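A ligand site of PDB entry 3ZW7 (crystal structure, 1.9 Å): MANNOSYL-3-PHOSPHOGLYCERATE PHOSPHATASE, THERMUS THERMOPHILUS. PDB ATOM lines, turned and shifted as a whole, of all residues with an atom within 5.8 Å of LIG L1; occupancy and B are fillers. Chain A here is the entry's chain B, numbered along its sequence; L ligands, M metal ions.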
ATOM      1  N   ASP A   6     -23.300   0.910  -4.456  1.00  0.00           N
ATOM      2  CA  ASP A   6     -22.442   1.390  -3.374  1.00  0.00           C
ATOM      3  C   ASP A   6     -21.069   1.651  -3.973  1.00  0.00           C
ATOM      4  O   ASP A   6     -20.767   1.145  -5.051  1.00  0.00           O
ATOM      5  CB  ASP A   6     -22.349   0.317  -2.294  1.00  0.00           C
ATOM      6  CG  ASP A   6     -21.947   0.878  -0.948  1.00  0.00           C
ATOM      7  OD1 ASP A   6     -21.402   2.010  -0.902  1.00  0.00           O
ATOM      8  OD2 ASP A   6     -22.188   0.210   0.077  1.00  0.00           O
ATOM      9  N   ASP A   8     -17.585   2.025  -1.741  1.00  0.00           N
ATOM     10  CA  ASP A   8     -16.609   1.227  -1.012  1.00  0.00           C
ATOM     11  C   ASP A   8     -17.011  -0.225  -0.933  1.00  0.00           C
ATOM     12  O   ASP A   8     -18.142  -0.545  -0.557  1.00  0.00           O
ATOM     13  CB  ASP A   8     -16.389   1.784   0.409  1.00  0.00           C
ATOM     14  CG  ASP A   8     -15.396   2.932   0.436  1.00  0.00           C
ATOM     15  OD1 ASP A   8     -14.520   2.982  -0.447  1.00  0.00           O
ATOM     16  OD2 ASP A   8     -15.495   3.784   1.347  1.00  0.00           O
ATOM     17  N   THR A  39     -23.798   6.085  -1.595  1.00  0.00           N
ATOM     18  CA  THR A  39     -22.603   5.840  -0.795  1.00  0.00           C
ATOM     19  C   THR A  39     -22.650   6.516   0.568  1.00  0.00           C
ATOM     20  O   THR A  39     -23.410   7.468   0.777  1.00  0.00           O
ATOM     21  CB  THR A  39     -21.382   6.395  -1.555  1.00  0.00           C
ATOM     22  OG1 THR A  39     -20.194   6.211  -0.790  1.00  0.00           O
ATOM     23  CG2 THR A  39     -21.547   7.888  -1.826  1.00  0.00           C
ATOM     24  N   ALA A  40     -21.813   6.036   1.487  1.00  0.00           N
ATOM     25  CA  ALA A  40     -21.562   6.704   2.763  1.00  0.00           C
ATOM     26  C   ALA A  40     -20.638   7.913   2.594  1.00  0.00           C
ATOM     27  O   ALA A  40     -20.514   8.745   3.494  1.00  0.00           O
ATOM     28  CB  ALA A  40     -20.939   5.722   3.761  1.00  0.00           C
ATOM     29  N   LYS A  41     -19.997   8.025   1.430  1.00  0.00           N
ATOM     30  CA  LYS A  41     -19.009   9.079   1.205  1.00  0.00           C
ATOM     31  C   LYS A  41     -19.637  10.468   1.081  1.00  0.00           C
ATOM     32  O   LYS A  41     -20.833  10.604   0.804  1.00  0.00           O
ATOM     33  CB  LYS A  41     -18.153   8.761  -0.024  1.00  0.00           C
ATOM     34  CG  LYS A  41     -17.304   7.496   0.148  1.00  0.00           C
ATOM     35  CD  LYS A  41     -16.526   7.177  -1.120  1.00  0.00           C
ATOM     36  CE  LYS A  41     -15.593   6.008  -0.908  1.00  0.00           C
ATOM     37  NZ  LYS A  41     -14.577   6.302   0.135  1.00  0.00           N
ATOM     38  N   THR A  42     -18.831  11.507   1.299  1.00  0.00           N
ATOM     39  CA  THR A  42     -19.312  12.875   1.175  1.00  0.00           C
ATOM     40  C   THR A  42     -19.253  13.316  -0.277  1.00  0.00           C
ATOM     41  O   THR A  42     -18.589  12.696  -1.106  1.00  0.00           O
ATOM     42  CB  THR A  42     -18.435  13.833   1.976  1.00  0.00           C
ATOM     43  OG1 THR A  42     -17.147  13.912   1.346  1.00  0.00           O
ATOM     44  CG2 THR A  42     -18.243  13.315   3.403  1.00  0.00           C
ATOM     45  N   GLU A  45     -15.742  13.738  -1.588  1.00  0.00           N
ATOM     46  CA  GLU A  45     -15.132  12.456  -1.929  1.00  0.00           C
ATOM     47  C   GLU A  45     -15.611  11.964  -3.291  1.00  0.00           C
ATOM     48  O   GLU A  45     -14.820  11.513  -4.121  1.00  0.00           O
ATOM     49  CB  GLU A  45     -15.459  11.405  -0.864  1.00  0.00           C
ATOM     50  CG  GLU A  45     -14.800  11.698   0.484  1.00  0.00           C
ATOM     51  CD  GLU A  45     -15.022  10.571   1.474  1.00  0.00           C
ATOM     52  OE1 GLU A  45     -16.160  10.467   1.989  1.00  0.00           O
ATOM     53  OE2 GLU A  45     -14.078   9.812   1.748  1.00  0.00           O
ATOM     54  N   TYR A 110     -15.598  11.673  13.426  1.00  0.00           N
ATOM     55  CA  TYR A 110     -14.661  12.417  12.596  1.00  0.00           C
ATOM     56  C   TYR A 110     -14.609  13.897  12.975  1.00  0.00           C
ATOM     57  O   TYR A 110     -13.555  14.535  12.905  1.00  0.00           O
ATOM     58  CB  TYR A 110     -15.048  12.344  11.116  1.00  0.00           C
ATOM     59  CG  TYR A 110     -14.702  11.061  10.402  1.00  0.00           C
ATOM     60  CD1 TYR A 110     -14.221   9.960  11.087  1.00  0.00           C
ATOM     61  CD2 TYR A 110     -14.851  10.964   9.021  1.00  0.00           C
ATOM     62  CE1 TYR A 110     -13.899   8.780  10.412  1.00  0.00           C
ATOM     63  CE2 TYR A 110     -14.538   9.788   8.348  1.00  0.00           C
ATOM     64  CZ  TYR A 110     -14.078   8.709   9.047  1.00  0.00           C
ATOM     65  OH  TYR A 110     -13.772   7.554   8.354  1.00  0.00           O
ATOM     66  N   THR A 122      -8.025   5.554   8.790  1.00  0.00           N
ATOM     67  CA  THR A 122      -8.761   5.067   7.630  1.00  0.00           C
ATOM     68  C   THR A 122      -7.835   4.537   6.547  1.00  0.00           C
ATOM     69  O   THR A 122      -8.292   3.855   5.626  1.00  0.00           O
ATOM     70  CB  THR A 122      -9.608   6.180   6.979  1.00  0.00           C
ATOM     71  OG1 THR A 122      -8.744   7.262   6.610  1.00  0.00           O
ATOM     72  CG2 THR A 122     -10.676   6.692   7.927  1.00  0.00           C
ATOM     73  N   LEU A 124      -6.443   6.490   4.546  1.00  0.00           N
ATOM     74  CA  LEU A 124      -6.523   7.513   3.509  1.00  0.00           C
ATOM     75  C   LEU A 124      -5.358   8.479   3.596  1.00  0.00           C
ATOM     76  O   LEU A 124      -4.738   8.618   4.655  1.00  0.00           O
ATOM     77  CB  LEU A 124      -7.828   8.289   3.623  1.00  0.00           C
ATOM     78  CG  LEU A 124      -9.127   7.525   3.378  1.00  0.00           C
ATOM     79  CD1 LEU A 124     -10.305   8.400   3.781  1.00  0.00           C
ATOM     80  CD2 LEU A 124      -9.248   7.097   1.915  1.00  0.00           C
ATOM     81  N   ALA A 132     -13.213  13.337   3.461  1.00  0.00           N
ATOM     82  CA  ALA A 132     -14.064  12.491   4.317  1.00  0.00           C
ATOM     83  C   ALA A 132     -14.611  13.225   5.541  1.00  0.00           C
ATOM     84  O   ALA A 132     -15.671  12.877   6.066  1.00  0.00           O
ATOM     85  CB  ALA A 132     -13.327  11.208   4.734  1.00  0.00           C
ATOM     86  N   ARG A 135     -18.348  16.664   6.059  1.00  0.00           N
ATOM     87  CA  ARG A 135     -19.635  15.973   6.087  1.00  0.00           C
ATOM     88  C   ARG A 135     -20.801  16.954   6.235  1.00  0.00           C
ATOM     89  O   ARG A 135     -20.704  17.927   6.972  1.00  0.00           O
ATOM     90  CB  ARG A 135     -19.634  14.937   7.233  1.00  0.00           C
ATOM     91  CG  ARG A 135     -18.358  14.104   7.269  1.00  0.00           C
ATOM     92  CD  ARG A 135     -18.521  12.808   8.069  1.00  0.00           C
ATOM     93  NE  ARG A 135     -19.433  11.845   7.446  1.00  0.00           N
ATOM     94  CZ  ARG A 135     -19.083  10.979   6.492  1.00  0.00           C
ATOM     95  NH1 ARG A 135     -17.852  10.976   5.992  1.00  0.00           N
ATOM     96  NH2 ARG A 135     -19.996  10.142   6.004  1.00  0.00           N
ATOM     97  N   THR A 140     -19.423   9.957  11.026  1.00  0.00           N
ATOM     98  CA  THR A 140     -18.745   8.674  11.125  1.00  0.00           C
ATOM     99  C   THR A 140     -18.196   8.564  12.533  1.00  0.00           C
ATOM    100  O   THR A 140     -17.432   9.439  12.988  1.00  0.00           O
ATOM    101  CB  THR A 140     -17.622   8.512  10.074  1.00  0.00           C
ATOM    102  OG1 THR A 140     -18.171   8.650   8.747  1.00  0.00           O
ATOM    103  CG2 THR A 140     -16.957   7.145  10.217  1.00  0.00           C
ATOM    104  N   HIS A 164     -24.133   0.929   9.801  1.00  0.00           N
ATOM    105  CA  HIS A 164     -22.726   0.565   9.712  1.00  0.00           C
ATOM    106  C   HIS A 164     -22.361   0.521   8.247  1.00  0.00           C
ATOM    107  O   HIS A 164     -23.094  -0.044   7.449  1.00  0.00           O
ATOM    108  CB  HIS A 164     -22.516  -0.790  10.365  1.00  0.00           C
ATOM    109  CG  HIS A 164     -21.070  -1.176  10.507  1.00  0.00           C
ATOM    110  ND1 HIS A 164     -20.400  -1.881   9.538  1.00  0.00           N
ATOM    111  CD2 HIS A 164     -20.181  -0.973  11.513  1.00  0.00           C
ATOM    112  CE1 HIS A 164     -19.153  -2.098   9.933  1.00  0.00           C
ATOM    113  NE2 HIS A 164     -19.010  -1.560  11.128  1.00  0.00           N
ATOM    114  N   GLY A 165     -21.223   1.113   7.885  1.00  0.00           N
ATOM    115  CA  GLY A 165     -20.884   1.257   6.493  1.00  0.00           C
ATOM    116  C   GLY A 165     -19.888   0.254   5.937  1.00  0.00           C
ATOM    117  O   GLY A 165     -19.510   0.331   4.760  1.00  0.00           O
ATOM    118  N   GLY A 166     -19.465  -0.699   6.761  1.00  0.00           N
ATOM    119  CA  GLY A 166     -18.443  -1.641   6.338  1.00  0.00           C
ATOM    120  C   GLY A 166     -17.272  -1.693   7.295  1.00  0.00           C
ATOM    121  O   GLY A 166     -16.776  -2.776   7.617  1.00  0.00           O
ATOM    122  N   ARG A 167     -16.830  -0.533   7.766  1.00  0.00           N
ATOM    123  CA  ARG A 167     -15.773  -0.467   8.777  1.00  0.00           C
ATOM    124  C   ARG A 167     -16.183   0.349  10.014  1.00  0.00           C
ATOM    125  O   ARG A 167     -15.795   0.033  11.134  1.00  0.00           O
ATOM    126  CB  ARG A 167     -14.469   0.080   8.181  1.00  0.00           C
ATOM    127  CG  ARG A 167     -13.880  -0.778   7.062  1.00  0.00           C
ATOM    128  CD  ARG A 167     -12.426  -0.416   6.786  1.00  0.00           C
ATOM    129  NE  ARG A 167     -12.277   0.942   6.267  1.00  0.00           N
ATOM    130  CZ  ARG A 167     -11.116   1.595   6.196  1.00  0.00           C
ATOM    131  NH1 ARG A 167      -9.997   1.015   6.600  1.00  0.00           N
ATOM    132  NH2 ARG A 167     -11.069   2.824   5.709  1.00  0.00           N
ATOM    133  N   PHE A 168     -16.978   1.393   9.806  1.00  0.00           N
ATOM    134  CA  PHE A 168     -17.361   2.279  10.903  1.00  0.00           C
ATOM    135  C   PHE A 168     -18.872   2.333  11.094  1.00  0.00           C
ATOM    136  O   PHE A 168     -19.625   2.179  10.148  1.00  0.00           O
ATOM    137  CB  PHE A 168     -16.891   3.706  10.607  1.00  0.00           C
ATOM    138  CG  PHE A 168     -15.409   3.830  10.439  1.00  0.00           C
ATOM    139  CD1 PHE A 168     -14.597   4.035  11.530  1.00  0.00           C
ATOM    140  CD2 PHE A 168     -14.843   3.744   9.180  1.00  0.00           C
ATOM    141  CE1 PHE A 168     -13.226   4.151  11.385  1.00  0.00           C
ATOM    142  CE2 PHE A 168     -13.477   3.857   9.016  1.00  0.00           C
ATOM    143  CZ  PHE A 168     -12.668   4.068  10.128  1.00  0.00           C
ATOM    144  N   TYR A 169     -19.298   2.603  12.336  1.00  0.00           N
ATOM    145  CA  TYR A 169     -20.672   3.014  12.610  1.00  0.00           C
ATOM    146  C   TYR A 169     -20.887   4.467  12.211  1.00  0.00           C
ATOM    147  O   TYR A 169     -19.965   5.276  12.259  1.00  0.00           O
ATOM    148  CB  TYR A 169     -21.013   2.813  14.091  1.00  0.00           C
ATOM    149  CG  TYR A 169     -21.072   1.345  14.447  1.00  0.00           C
ATOM    150  CD1 TYR A 169     -22.257   0.641  14.331  1.00  0.00           C
ATOM    151  CD2 TYR A 169     -19.942   0.669  14.879  1.00  0.00           C
ATOM    152  CE1 TYR A 169     -22.326  -0.706  14.626  1.00  0.00           C
ATOM    153  CE2 TYR A 169     -19.993  -0.694  15.180  1.00  0.00           C
ATOM    154  CZ  TYR A 169     -21.198  -1.361  15.056  1.00  0.00           C
ATOM    155  OH  TYR A 169     -21.278  -2.705  15.343  1.00  0.00           O
ATOM    156  N   HIS A 170     -22.107   4.772  11.821  1.00  0.00           N
ATOM    157  CA  HIS A 170     -22.480   6.140  11.466  1.00  0.00           C
ATOM    158  C   HIS A 170     -23.696   6.578  12.267  1.00  0.00           C
ATOM    159  O   HIS A 170     -24.531   5.770  12.643  1.00  0.00           O
ATOM    160  CB  HIS A 170     -22.854   6.181   9.982  1.00  0.00           C
ATOM    161  CG  HIS A 170     -21.689   6.009   9.066  1.00  0.00           C
ATOM    162  ND1 HIS A 170     -21.122   7.059   8.379  1.00  0.00           N
ATOM    163  CD2 HIS A 170     -20.992   4.902   8.734  1.00  0.00           C
ATOM    164  CE1 HIS A 170     -20.114   6.606   7.663  1.00  0.00           C
ATOM    165  NE2 HIS A 170     -20.012   5.304   7.851  1.00  0.00           N
ATOM    166  N   ASN A 205     -25.478  -0.656   5.721  1.00  0.00           N
ATOM    167  CA  ASN A 205     -26.162   0.530   5.193  1.00  0.00           C
ATOM    168  C   ASN A 205     -26.823   0.298   3.820  1.00  0.00           C
ATOM    169  O   ASN A 205     -27.562   1.144   3.330  1.00  0.00           O
ATOM    170  CB  ASN A 205     -25.213   1.754   5.142  1.00  0.00           C
ATOM    171  CG  ASN A 205     -23.960   1.493   4.324  1.00  0.00           C
ATOM    172  OD1 ASN A 205     -23.753   0.398   3.801  1.00  0.00           O
ATOM    173  ND2 ASN A 205     -23.129   2.516   4.190  1.00  0.00           N
HETATM  174  C1  LIG L   1     -16.769   5.848   5.906  1.00  0.00           C
HETATM  175  O1  LIG L   1     -17.538   5.038   5.017  1.00  0.00           O
HETATM  176  C2  LIG L   1     -17.128   3.669   4.953  1.00  0.00           C
HETATM  177  C3  LIG L   1     -17.809   3.023   3.749  1.00  0.00           C
HETATM  178  O2  LIG L   1     -17.657   3.910   2.625  1.00  0.00           O
HETATM  179  C4  LIG L   1     -17.481   2.916   6.207  1.00  0.00           C
HETATM  180  O3  LIG L   1     -18.375   3.364   6.943  1.00  0.00           O
HETATM  181  O4  LIG L   1     -17.071   1.742   6.302  1.00  0.00           O
HETATM  182  C5  LIG L   1     -17.094   7.310   5.623  1.00  0.00           C
HETATM  183  O5  LIG L   1     -16.467   8.100   6.640  1.00  0.00           O
HETATM  184  C6  LIG L   1     -16.592   7.723   4.251  1.00  0.00           C
HETATM  185  O6  LIG L   1     -16.781   9.117   4.091  1.00  0.00           O
HETATM  186  C7  LIG L   1     -15.094   7.430   4.139  1.00  0.00           C
HETATM  187  O7  LIG L   1     -14.615   7.632   2.805  1.00  0.00           O
HETATM  188  C8  LIG L   1     -14.781   5.990   4.508  1.00  0.00           C
HETATM  189  C9  LIG L   1     -13.274   5.817   4.581  1.00  0.00           C
HETATM  190  O8  LIG L   1     -12.987   4.439   4.836  1.00  0.00           O
HETATM  191  O9  LIG L   1     -15.358   5.610   5.752  1.00  0.00           O
HETATM  192  P1  LG2 L   2     -19.832   3.278   1.182  1.00  0.00           P
HETATM  193  O1  LG2 L   2     -21.295   3.116   1.569  1.00  0.00           O
HETATM  194  O2  LG2 L   2     -19.557   3.901  -0.162  1.00  0.00           O
HETATM  195  O3  LG2 L   2     -19.106   1.956   1.229  1.00  0.00           O
HETATM  196 MG    MG M   1     -19.952  -0.105   1.403  1.00  0.00          MG
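An oxygen (O3) of LIG L1 lies within hydrogen-bond range of a ring nitrogen (NE2) of His 170, at 2.7 Å.
The backbone NH (N) of Asp 8 sits at hydrogen-bond distance from an oxygen (O2) of LG2 L2, at 3.1 Å.
An oxygen (O1) of LG2 L2 lies within hydrogen-bond range of the backbone NH (N) of Ala 40, at 3.0 Å.
The side-chain carboxylate of Glu 45 sits at hydrogen-bond distance from an oxygen (O7) of LIG L1, at 2.5 Å.
N of Gly 166 is in hydrogen-bond range of O4 of LIG L1.
O6 of LIG L1 lies within hydrogen-bond range of NH1 of Arg 135 (2.9 Å).
O2 of LG2 L2 sits at hydrogen-bond distance from OG1 of Thr 39 (2.5 Å).
O7 of LIG L1 is in hydrogen-bond range of NZ of Lys 41 (3.0 Å).
An oxygen (O4) of LIG L1 is in hydrogen-bond range of the backbone NH of Arg 167 (2.7 Å).
An oxygen (O2) of LIG L1 lies within hydrogen-bond range of the side-chain carboxylate (OD2) of Asp 8 (2.5 Å).
An oxygen (O8) of LIG L1 sits at hydrogen-bond distance from the guanidinium group (NH2) of Arg 167 (2.7 Å).
The side-chain amide nitrogen (ND2) of Asn 205 sits at hydrogen-bond distance from an oxygen (O1) of LG2 L2 (3.3 Å).
The side-chain hydroxyl (OG1) of Thr 140 sits at hydrogen-bond distance from an oxygen (O5) of LIG L1.
The side-chain hydroxyl (OH) of Tyr 110 lies close to an oxygen (O5) of LIG L1 (3.2 Å).
The side-chain carboxylate (OD1) of Asp 6 sits close to an oxygen (O1) of LG2 L2.
An oxygen (O2) of LG2 L2 lies within hydrogen-bond range of an oxygen (O2) of LIG L1 (3.4 Å).
The side-chain hydroxyl (OG1) of Thr 140 sits close to a ring nitrogen (ND1) of His 170 (3.4 Å).
The backbone NH (N) of Gly 166 sits at hydrogen-bond distance from a ring nitrogen (ND1) of His 164, at 3.2 Å.
OE2 of Glu 45 is in salt-bridge range of NZ of Lys 41 (3.9 Å).
The guanidinium group (NH1) of Arg 135 sits at hydrogen-bond distance from the backbone carbonyl oxygen (O) of Ala 132, 2.9 Å away.
The side-chain carboxylate (OE1) of Glu 45 lies within hydrogen-bond range of the backbone NH (N) of Thr 42 (2.9 Å).
The side-chain carboxylate of Asp 8 is in salt-bridge range of the side-chain amino group of Lys 41.
The side-chain hydroxyl of Thr 39 sits at hydrogen-bond distance from the backbone NH of Lys 41, 2.9 Å away.
N of Tyr 110 is in hydrogen-bond range of O of Thr 140 (2.9 Å).
The backbone carbonyl oxygen (O) of Gly 165 lies close to an oxygen (O4) of LIG L1, at 3.2 Å.
Ala 40 touches LIG L1 (CB to O1, 3.7 Å).
Phe 168 touches LIG L1 (N to O4, 3.5 Å).
Hydrophobic or aromatic side chains within 4 Å of LIG L1: Ala 40, Tyr 110, Phe 168 and His 170.
Within 4 Å of LIG L1: Asp 8, Ala 40, Lys 41, Glu 45, Tyr 110, Arg 135, Thr 140, Gly 165, Gly 166, Arg 167, Phe 168 and His 170.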
